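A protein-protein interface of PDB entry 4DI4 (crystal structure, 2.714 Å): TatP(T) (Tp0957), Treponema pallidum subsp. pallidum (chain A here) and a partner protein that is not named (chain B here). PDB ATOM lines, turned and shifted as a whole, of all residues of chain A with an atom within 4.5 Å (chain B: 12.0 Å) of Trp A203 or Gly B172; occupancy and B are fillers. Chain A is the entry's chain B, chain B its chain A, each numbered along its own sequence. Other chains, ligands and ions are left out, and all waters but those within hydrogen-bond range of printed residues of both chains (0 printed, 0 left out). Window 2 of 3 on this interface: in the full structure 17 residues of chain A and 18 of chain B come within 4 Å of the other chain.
Among the printed residues, pairs that only touch across the chains: Leu A200 with Leu B171 (3.95 Å), Leu A200 with Gly B172 (3.96 Å), Trp A203 with Pro B176 (3.996 Å), Ala A204 with Pro B176 (3.5 Å), Ala A204 with Phe B216 (3.6 Å) and Gly A206 with Pro B176 (3.6 Å).
Printed residues of chain B within 4 Å of Trp A203: Gly B172 and Pro B176. Of chain A, only Leu A200 and Trp A203 come within 4 Å of Gly B172. Leu A200 touches just these residues of chain B: Leu B171 (3.95 Å) and Gly B172 (3.96 Å). No residue of chain B comes within 4 Å of Thr A202. Ala A204 touches just these residues of chain B: Pro B176 and Phe B216. No residue of chain B comes within 4 Å of Thr A205. Of chain B, only Pro B176 (3.6 Å) comes within 4 Å of Gly A206. No residue of chain B comes within 4 Å of Tyr A208. No residue of chain B comes within 4 Å of Asn A269. Of the printed residues of chain A, Phe B216 touches Ala A204 (3.6 Å). Printed residues of chain A within 4 Å of Leu B171: Leu A200 (3.95 Å). Of the printed residues of chain A, Pro B176 touches Trp A203 (3.996 Å), Ala A204 (3.5 Å) and Gly A206 (3.6 Å).
Of the 22 printed residues of chain B, 4 touch a printed residue of chain A. Hydrophobic or aromatic side chains of chain B that line the printed part of chain A: Pro B176 and Phe B216. Printed residues of chain A that touch a printed residue of chain B: Leu A200, Trp A203, Ala A204 and Gly A206. Among the printed residues, 7 pairs touch across the chains. Among the printed residues, no Asp or Glu carboxylate lies within 4 Å of a Lys or Arg side-chain nitrogen of the other chain.
The backbone carbonyl oxygen of Gly B172 sits at hydrogen-bond distance from the indole nitrogen of Trp A203, at 3.2 Å.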
ATOM      1  N   HIS A 199      32.534  -3.608  12.360  1.00  0.00           N
ATOM      2  CA  HIS A 199      32.436  -2.158  12.570  1.00  0.00           C
ATOM      3  C   HIS A 199      31.417  -1.447  11.677  1.00  0.00           C
ATOM      4  O   HIS A 199      30.769  -0.502  12.111  1.00  0.00           O
ATOM      5  CB  HIS A 199      33.812  -1.480  12.420  1.00  0.00           C
ATOM      6  CG  HIS A 199      34.621  -1.469  13.686  1.00  0.00           C
ATOM      7  ND1 HIS A 199      34.173  -2.027  14.857  1.00  0.00           N
ATOM      8  CD2 HIS A 199      35.852  -0.959  13.940  1.00  0.00           C
ATOM      9  CE1 HIS A 199      35.103  -1.870  15.797  1.00  0.00           C
ATOM     10  NE2 HIS A 199      36.120  -1.224  15.266  1.00  0.00           N
ATOM     11  N   LEU A 200      31.296  -1.891  10.430  1.00  0.00           N
ATOM     12  CA  LEU A 200      30.421  -1.230   9.469  1.00  0.00           C
ATOM     13  C   LEU A 200      28.967  -1.444   9.845  1.00  0.00           C
ATOM     14  O   LEU A 200      28.128  -0.559   9.676  1.00  0.00           O
ATOM     15  CB  LEU A 200      30.680  -1.764   8.071  1.00  0.00           C
ATOM     16  CG  LEU A 200      30.045  -1.056   6.875  1.00  0.00           C
ATOM     17  CD1 LEU A 200      30.633   0.343   6.650  1.00  0.00           C
ATOM     18  CD2 LEU A 200      30.211  -1.905   5.632  1.00  0.00           C
ATOM     19  N   PHE A 201      28.682  -2.625  10.377  1.00  0.00           N
ATOM     20  CA  PHE A 201      27.350  -2.938  10.872  1.00  0.00           C
ATOM     21  C   PHE A 201      26.984  -2.037  12.048  1.00  0.00           C
ATOM     22  O   PHE A 201      25.963  -1.362  12.019  1.00  0.00           O
ATOM     23  CB  PHE A 201      27.247  -4.420  11.280  1.00  0.00           C
ATOM     24  CG  PHE A 201      25.957  -4.775  11.979  1.00  0.00           C
ATOM     25  CD1 PHE A 201      24.956  -5.461  11.305  1.00  0.00           C
ATOM     26  CD2 PHE A 201      25.742  -4.413  13.310  1.00  0.00           C
ATOM     27  CE1 PHE A 201      23.763  -5.790  11.945  1.00  0.00           C
ATOM     28  CE2 PHE A 201      24.559  -4.743  13.958  1.00  0.00           C
ATOM     29  CZ  PHE A 201      23.564  -5.429  13.278  1.00  0.00           C
ATOM     30  N   THR A 202      27.829  -2.031  13.072  1.00  0.00           N
ATOM     31  CA  THR A 202      27.518  -1.325  14.303  1.00  0.00           C
ATOM     32  C   THR A 202      27.472   0.195  14.080  1.00  0.00           C
ATOM     33  O   THR A 202      26.671   0.896  14.689  1.00  0.00           O
ATOM     34  CB  THR A 202      28.489  -1.704  15.437  1.00  0.00           C
ATOM     35  OG1 THR A 202      29.760  -1.098  15.199  1.00  0.00           O
ATOM     36  CG2 THR A 202      28.675  -3.203  15.478  1.00  0.00           C
ATOM     37  N   TRP A 203      28.296   0.698  13.173  1.00  0.00           N
ATOM     38  CA  TRP A 203      28.170   2.084  12.791  1.00  0.00           C
ATOM     39  C   TRP A 203      26.919   2.294  11.953  1.00  0.00           C
ATOM     40  O   TRP A 203      25.960   2.892  12.413  1.00  0.00           O
ATOM     41  CB  TRP A 203      29.383   2.563  12.020  1.00  0.00           C
ATOM     42  CG  TRP A 203      29.191   3.965  11.500  1.00  0.00           C
ATOM     43  CD1 TRP A 203      29.121   4.349  10.210  1.00  0.00           C
ATOM     44  CD2 TRP A 203      29.036   5.148  12.281  1.00  0.00           C
ATOM     45  NE1 TRP A 203      28.949   5.693  10.120  1.00  0.00           N
ATOM     46  CE2 TRP A 203      28.876   6.215  11.381  1.00  0.00           C
ATOM     47  CE3 TRP A 203      28.997   5.407  13.657  1.00  0.00           C
ATOM     48  CZ2 TRP A 203      28.687   7.530  11.804  1.00  0.00           C
ATOM     49  CZ3 TRP A 203      28.823   6.713  14.077  1.00  0.00           C
ATOM     50  CH2 TRP A 203      28.674   7.758  13.151  1.00  0.00           C
ATOM     51  N   ALA A 204      26.901   1.759  10.744  1.00  0.00           N
ATOM     52  CA  ALA A 204      25.817   2.044   9.806  1.00  0.00           C
ATOM     53  C   ALA A 204      24.385   1.801  10.340  1.00  0.00           C
ATOM     54  O   ALA A 204      23.430   2.401   9.829  1.00  0.00           O
ATOM     55  CB  ALA A 204      26.042   1.304   8.490  1.00  0.00           C
ATOM     56  N   THR A 205      24.224   0.950  11.353  1.00  0.00           N
ATOM     57  CA  THR A 205      22.883   0.687  11.889  1.00  0.00           C
ATOM     58  C   THR A 205      22.460   1.655  13.000  1.00  0.00           C
ATOM     59  O   THR A 205      21.316   1.635  13.439  1.00  0.00           O
ATOM     60  CB  THR A 205      22.749  -0.747  12.457  1.00  0.00           C
ATOM     61  OG1 THR A 205      23.584  -0.897  13.618  1.00  0.00           O
ATOM     62  CG2 THR A 205      23.108  -1.794  11.411  1.00  0.00           C
ATOM     63  N   GLY A 206      23.388   2.479  13.471  1.00  0.00           N
ATOM     64  CA  GLY A 206      23.156   3.265  14.663  1.00  0.00           C
ATOM     65  C   GLY A 206      23.201   2.447  15.955  1.00  0.00           C
ATOM     66  O   GLY A 206      23.005   2.992  17.042  1.00  0.00           O
ATOM     67  N   TYR A 208      25.612   1.411  17.552  1.00  0.00           N
ATOM     68  CA  TYR A 208      26.605   1.982  18.454  1.00  0.00           C
ATOM     69  C   TYR A 208      25.982   2.807  19.598  1.00  0.00           C
ATOM     70  O   TYR A 208      26.526   2.836  20.704  1.00  0.00           O
ATOM     71  CB  TYR A 208      27.598   2.836  17.675  1.00  0.00           C
ATOM     72  CG  TYR A 208      26.984   4.066  17.046  1.00  0.00           C
ATOM     73  CD1 TYR A 208      27.079   5.302  17.664  1.00  0.00           C
ATOM     74  CD2 TYR A 208      26.319   3.987  15.825  1.00  0.00           C
ATOM     75  CE1 TYR A 208      26.536   6.435  17.078  1.00  0.00           C
ATOM     76  CE2 TYR A 208      25.771   5.107  15.232  1.00  0.00           C
ATOM     77  CZ  TYR A 208      25.877   6.334  15.869  1.00  0.00           C
ATOM     78  OH  TYR A 208      25.326   7.460  15.295  1.00  0.00           O
ATOM     79  N   CYS A 266      34.978   3.900  10.375  1.00  0.00           N
ATOM     80  CA  CYS A 266      33.870   3.468  11.210  1.00  0.00           C
ATOM     81  C   CYS A 266      34.247   3.488  12.681  1.00  0.00           C
ATOM     82  O   CYS A 266      33.403   3.687  13.548  1.00  0.00           O
ATOM     83  CB  CYS A 266      33.366   2.094  10.795  1.00  0.00           C
ATOM     84  SG  CYS A 266      32.458   2.132   9.257  1.00  0.00           S
ATOM     85  N   ASN A 269      34.295   7.285  13.832  1.00  0.00           N
ATOM     86  CA  ASN A 269      32.909   7.700  13.969  1.00  0.00           C
ATOM     87  C   ASN A 269      32.233   7.103  15.173  1.00  0.00           C
ATOM     88  O   ASN A 269      31.439   7.758  15.837  1.00  0.00           O
ATOM     89  CB  ASN A 269      32.122   7.329  12.730  1.00  0.00           C
ATOM     90  CG  ASN A 269      32.402   8.248  11.601  1.00  0.00           C
ATOM     91  OD1 ASN A 269      33.511   8.768  11.471  1.00  0.00           O
ATOM     92  ND2 ASN A 269      31.398   8.487  10.779  1.00  0.00           N
ATOM     93  N   ILE A 270      32.519   5.838  15.443  1.00  0.00           N
ATOM     94  CA  ILE A 270      32.040   5.231  16.676  1.00  0.00           C
ATOM     95  C   ILE A 270      32.626   5.978  17.885  1.00  0.00           C
ATOM     96  O   ILE A 270      31.943   6.206  18.882  1.00  0.00           O
ATOM     97  CB  ILE A 270      32.375   3.730  16.717  1.00  0.00           C
ATOM     98  CG1 ILE A 270      31.311   2.946  15.952  1.00  0.00           C
ATOM     99  CG2 ILE A 270      32.451   3.219  18.138  1.00  0.00           C
ATOM    100  CD1 ILE A 270      31.786   1.570  15.457  1.00  0.00           C
ATOM    101  N   ARG B 107      23.051  12.439  -5.873  1.00  0.00           N
ATOM    102  CA  ARG B 107      22.943  12.382  -4.429  1.00  0.00           C
ATOM    103  C   ARG B 107      23.106  13.794  -3.876  1.00  0.00           C
ATOM    104  O   ARG B 107      22.378  14.211  -2.983  1.00  0.00           O
ATOM    105  CB  ARG B 107      24.035  11.469  -3.866  1.00  0.00           C
ATOM    106  CG  ARG B 107      23.970  11.188  -2.384  1.00  0.00           C
ATOM    107  CD  ARG B 107      25.315  10.754  -1.855  1.00  0.00           C
ATOM    108  NE  ARG B 107      26.221  11.890  -1.714  1.00  0.00           N
ATOM    109  CZ  ARG B 107      26.496  12.485  -0.554  1.00  0.00           C
ATOM    110  NH1 ARG B 107      25.941  12.054   0.583  1.00  0.00           N
ATOM    111  NH2 ARG B 107      27.333  13.514  -0.529  1.00  0.00           N
ATOM    112  N   SER B 134      18.251  16.661  15.978  1.00  0.00           N
ATOM    113  CA  SER B 134      18.830  16.489  17.303  1.00  0.00           C
ATOM    114  C   SER B 134      19.384  15.080  17.542  1.00  0.00           C
ATOM    115  O   SER B 134      20.479  14.909  18.086  1.00  0.00           O
ATOM    116  CB  SER B 134      17.807  16.834  18.389  1.00  0.00           C
ATOM    117  OG  SER B 134      16.674  15.996  18.327  1.00  0.00           O
ATOM    118  N   GLY B 135      18.625  14.069  17.140  1.00  0.00           N
ATOM    119  CA  GLY B 135      18.948  12.715  17.524  1.00  0.00           C
ATOM    120  C   GLY B 135      18.193  12.331  18.783  1.00  0.00           C
ATOM    121  O   GLY B 135      18.294  11.204  19.277  1.00  0.00           O
ATOM    122  N   ALA B 165      18.493  10.673  -1.502  1.00  0.00           N
ATOM    123  CA  ALA B 165      19.942  10.768  -1.319  1.00  0.00           C
ATOM    124  C   ALA B 165      20.484   9.497  -0.671  1.00  0.00           C
ATOM    125  O   ALA B 165      21.518   8.968  -1.058  1.00  0.00           O
ATOM    126  CB  ALA B 165      20.325  11.985  -0.481  1.00  0.00           C
ATOM    127  N   PHE B 166      19.774   9.024   0.335  1.00  0.00           N
ATOM    128  CA  PHE B 166      20.251   7.924   1.124  1.00  0.00           C
ATOM    129  C   PHE B 166      20.393   6.684   0.219  1.00  0.00           C
ATOM    130  O   PHE B 166      21.285   5.853   0.385  1.00  0.00           O
ATOM    131  CB  PHE B 166      19.283   7.704   2.299  1.00  0.00           C
ATOM    132  CG  PHE B 166      19.451   6.368   2.987  1.00  0.00           C
ATOM    133  CD1 PHE B 166      20.531   6.136   3.847  1.00  0.00           C
ATOM    134  CD2 PHE B 166      18.527   5.334   2.765  1.00  0.00           C
ATOM    135  CE1 PHE B 166      20.668   4.908   4.484  1.00  0.00           C
ATOM    136  CE2 PHE B 166      18.662   4.102   3.393  1.00  0.00           C
ATOM    137  CZ  PHE B 166      19.731   3.891   4.263  1.00  0.00           C
ATOM    138  N   ALA B 167      19.515   6.588  -0.764  1.00  0.00           N
ATOM    139  CA  ALA B 167      19.499   5.441  -1.631  1.00  0.00           C
ATOM    140  C   ALA B 167      20.719   5.427  -2.575  1.00  0.00           C
ATOM    141  O   ALA B 167      21.057   4.384  -3.154  1.00  0.00           O
ATOM    142  CB  ALA B 167      18.201   5.422  -2.412  1.00  0.00           C
ATOM    143  N   LEU B 168      21.316   6.601  -2.783  1.00  0.00           N
ATOM    144  CA  LEU B 168      22.528   6.775  -3.593  1.00  0.00           C
ATOM    145  C   LEU B 168      23.799   6.920  -2.760  1.00  0.00           C
ATOM    146  O   LEU B 168      24.852   7.358  -3.252  1.00  0.00           O
ATOM    147  CB  LEU B 168      22.392   7.905  -4.613  1.00  0.00           C
ATOM    148  CG  LEU B 168      21.192   7.829  -5.552  1.00  0.00           C
ATOM    149  CD1 LEU B 168      21.225   8.982  -6.589  1.00  0.00           C
ATOM    150  CD2 LEU B 168      21.122   6.444  -6.194  1.00  0.00           C
ATOM    151  N   THR B 169      23.667   6.655  -1.476  1.00  0.00           N
ATOM    152  CA  THR B 169      24.746   6.921  -0.545  1.00  0.00           C
ATOM    153  C   THR B 169      25.508   5.644  -0.173  1.00  0.00           C
ATOM    154  O   THR B 169      24.903   4.661   0.258  1.00  0.00           O
ATOM    155  CB  THR B 169      24.173   7.628   0.703  1.00  0.00           C
ATOM    156  OG1 THR B 169      23.758   8.932   0.309  1.00  0.00           O
ATOM    157  CG2 THR B 169      25.198   7.750   1.806  1.00  0.00           C
ATOM    158  N   PRO B 170      26.842   5.658  -0.343  1.00  0.00           N
ATOM    159  CA  PRO B 170      27.714   4.521  -0.006  1.00  0.00           C
ATOM    160  C   PRO B 170      27.467   4.053   1.412  1.00  0.00           C
ATOM    161  O   PRO B 170      27.383   4.869   2.327  1.00  0.00           O
ATOM    162  CB  PRO B 170      29.118   5.110  -0.103  1.00  0.00           C
ATOM    163  CG  PRO B 170      28.978   6.222  -1.086  1.00  0.00           C
ATOM    164  CD  PRO B 170      27.611   6.811  -0.833  1.00  0.00           C
ATOM    165  N   LEU B 171      27.335   2.745   1.576  1.00  0.00           N
ATOM    166  CA  LEU B 171      27.056   2.135   2.862  1.00  0.00           C
ATOM    167  C   LEU B 171      28.094   2.592   3.865  1.00  0.00           C
ATOM    168  O   LEU B 171      29.295   2.495   3.616  1.00  0.00           O
ATOM    169  CB  LEU B 171      27.124   0.630   2.712  1.00  0.00           C
ATOM    170  CG  LEU B 171      26.775  -0.292   3.868  1.00  0.00           C
ATOM    171  CD1 LEU B 171      25.373   0.010   4.350  1.00  0.00           C
ATOM    172  CD2 LEU B 171      26.904  -1.745   3.381  1.00  0.00           C
ATOM    173  N   GLY B 172      27.628   3.098   5.003  1.00  0.00           N
ATOM    174  CA  GLY B 172      28.518   3.635   6.014  1.00  0.00           C
ATOM    175  C   GLY B 172      28.669   5.141   5.948  1.00  0.00           C
ATOM    176  O   GLY B 172      29.140   5.757   6.897  1.00  0.00           O
ATOM    177  N   SER B 173      28.286   5.736   4.823  1.00  0.00           N
ATOM    178  CA  SER B 173      28.382   7.182   4.665  1.00  0.00           C
ATOM    179  C   SER B 173      27.138   7.939   5.138  1.00  0.00           C
ATOM    180  O   SER B 173      27.205   9.139   5.359  1.00  0.00           O
ATOM    181  CB  SER B 173      28.701   7.550   3.222  1.00  0.00           C
ATOM    182  OG  SER B 173      29.976   7.066   2.861  1.00  0.00           O
ATOM    183  N   ALA B 174      26.020   7.242   5.325  1.00  0.00           N
ATOM    184  CA  ALA B 174      24.824   7.903   5.833  1.00  0.00           C
ATOM    185  C   ALA B 174      24.935   8.157   7.338  1.00  0.00           C
ATOM    186  O   ALA B 174      25.866   7.701   7.996  1.00  0.00           O
ATOM    187  CB  ALA B 174      23.582   7.064   5.527  1.00  0.00           C
ATOM    188  N   LEU B 175      23.975   8.894   7.880  1.00  0.00           N
ATOM    189  CA  LEU B 175      23.870   9.080   9.318  1.00  0.00           C
ATOM    190  C   LEU B 175      22.510   8.518   9.695  1.00  0.00           C
ATOM    191  O   LEU B 175      21.483   9.030   9.249  1.00  0.00           O
ATOM    192  CB  LEU B 175      23.980  10.563   9.678  1.00  0.00           C
ATOM    193  CG  LEU B 175      24.810  11.003  10.895  1.00  0.00           C
ATOM    194  CD1 LEU B 175      24.306  10.397  12.228  1.00  0.00           C
ATOM    195  CD2 LEU B 175      26.289  10.708  10.670  1.00  0.00           C
ATOM    196  N   PRO B 176      22.489   7.445  10.491  1.00  0.00           N
ATOM    197  CA  PRO B 176      21.199   6.777  10.690  1.00  0.00           C
ATOM    198  C   PRO B 176      20.106   7.717  11.226  1.00  0.00           C
ATOM    199  O   PRO B 176      18.936   7.516  10.880  1.00  0.00           O
ATOM    200  CB  PRO B 176      21.531   5.673  11.693  1.00  0.00           C
ATOM    201  CG  PRO B 176      23.009   5.436  11.526  1.00  0.00           C
ATOM    202  CD  PRO B 176      23.594   6.771  11.196  1.00  0.00           C
ATOM    203  N   ASP B 177      20.479   8.723  12.023  1.00  0.00           N
ATOM    204  CA  ASP B 177      19.509   9.670  12.586  1.00  0.00           C
ATOM    205  C   ASP B 177      18.897  10.565  11.525  1.00  0.00           C
ATOM    206  O   ASP B 177      17.725  10.928  11.601  1.00  0.00           O
ATOM    207  CB  ASP B 177      20.156  10.553  13.646  1.00  0.00           C
ATOM    208  CG  ASP B 177      20.760   9.756  14.783  1.00  0.00           C
ATOM    209  OD1 ASP B 177      21.026   8.540  14.606  1.00  0.00           O
ATOM    210  OD2 ASP B 177      20.987  10.359  15.854  1.00  0.00           O
ATOM    211  N   THR B 178      19.709  10.941  10.547  1.00  0.00           N
ATOM    212  CA  THR B 178      19.244  11.781   9.460  1.00  0.00           C
ATOM    213  C   THR B 178      18.173  11.060   8.660  1.00  0.00           C
ATOM    214  O   THR B 178      17.133  11.640   8.327  1.00  0.00           O
ATOM    215  CB  THR B 178      20.414  12.234   8.561  1.00  0.00           C
ATOM    216  OG1 THR B 178      21.332  13.003   9.345  1.00  0.00           O
ATOM    217  CG2 THR B 178      19.922  13.099   7.423  1.00  0.00           C
ATOM    218  N   VAL B 179      18.422   9.788   8.370  1.00  0.00           N
ATOM    219  CA  VAL B 179      17.457   8.971   7.654  1.00  0.00           C
ATOM    220  C   VAL B 179      16.180   8.858   8.474  1.00  0.00           C
ATOM    221  O   VAL B 179      15.083   9.180   8.005  1.00  0.00           O
ATOM    222  CB  VAL B 179      18.020   7.570   7.371  1.00  0.00           C
ATOM    223  CG1 VAL B 179      17.153   6.833   6.366  1.00  0.00           C
ATOM    224  CG2 VAL B 179      19.429   7.687   6.840  1.00  0.00           C
ATOM    225  N   HIS B 180      16.325   8.419   9.713  1.00  0.00           N
ATOM    226  CA  HIS B 180      15.170   8.304  10.581  1.00  0.00           C
ATOM    227  C   HIS B 180      14.330   9.605  10.620  1.00  0.00           C
ATOM    228  O   HIS B 180      13.093   9.565  10.553  1.00  0.00           O
ATOM    229  CB  HIS B 180      15.586   7.866  11.984  1.00  0.00           C
ATOM    230  CG  HIS B 180      14.436   7.756  12.932  1.00  0.00           C
ATOM    231  ND1 HIS B 180      13.560   6.688  12.919  1.00  0.00           N
ATOM    232  CD2 HIS B 180      13.983   8.598  13.891  1.00  0.00           C
ATOM    233  CE1 HIS B 180      12.634   6.872  13.836  1.00  0.00           C
ATOM    234  NE2 HIS B 180      12.863   8.028  14.439  1.00  0.00           N
ATOM    235  N   PRO B 213      16.065  -2.950   5.979  1.00  0.00           N
ATOM    236  CA  PRO B 213      15.886  -4.140   6.827  1.00  0.00           C
ATOM    237  C   PRO B 213      14.900  -3.877   7.949  1.00  0.00           C
ATOM    238  O   PRO B 213      14.695  -2.720   8.327  1.00  0.00           O
ATOM    239  CB  PRO B 213      17.285  -4.386   7.420  1.00  0.00           C
ATOM    240  CG  PRO B 213      18.221  -3.543   6.595  1.00  0.00           C
ATOM    241  CD  PRO B 213      17.411  -2.372   6.105  1.00  0.00           C
ATOM    242  N   SER B 215      15.429  -4.108  10.693  1.00  0.00           N
ATOM    243  CA  SER B 215      16.284  -3.468  11.697  1.00  0.00           C
ATOM    244  C   SER B 215      16.636  -1.998  11.400  1.00  0.00           C
ATOM    245  O   SER B 215      17.225  -1.311  12.236  1.00  0.00           O
ATOM    246  CB  SER B 215      17.573  -4.283  11.877  1.00  0.00           C
ATOM    247  OG  SER B 215      18.266  -4.437  10.647  1.00  0.00           O
ATOM    248  N   PHE B 216      16.329  -1.541  10.192  1.00  0.00           N
ATOM    249  CA  PHE B 216      16.524  -0.136   9.827  1.00  0.00           C
ATOM    250  C   PHE B 216      15.272   0.731   9.851  1.00  0.00           C
ATOM    251  O   PHE B 216      15.285   1.857   9.344  1.00  0.00           O
ATOM    252  CB  PHE B 216      17.204   0.002   8.477  1.00  0.00           C
ATOM    253  CG  PHE B 216      18.063   1.221   8.371  1.00  0.00           C
ATOM    254  CD1 PHE B 216      19.045   1.470   9.321  1.00  0.00           C
ATOM    255  CD2 PHE B 216      17.904   2.110   7.331  1.00  0.00           C
ATOM    256  CE1 PHE B 216      19.864   2.583   9.236  1.00  0.00           C
ATOM    257  CE2 PHE B 216      18.721   3.223   7.235  1.00  0.00           C
ATOM    258  CZ  PHE B 216      19.702   3.460   8.195  1.00  0.00           C
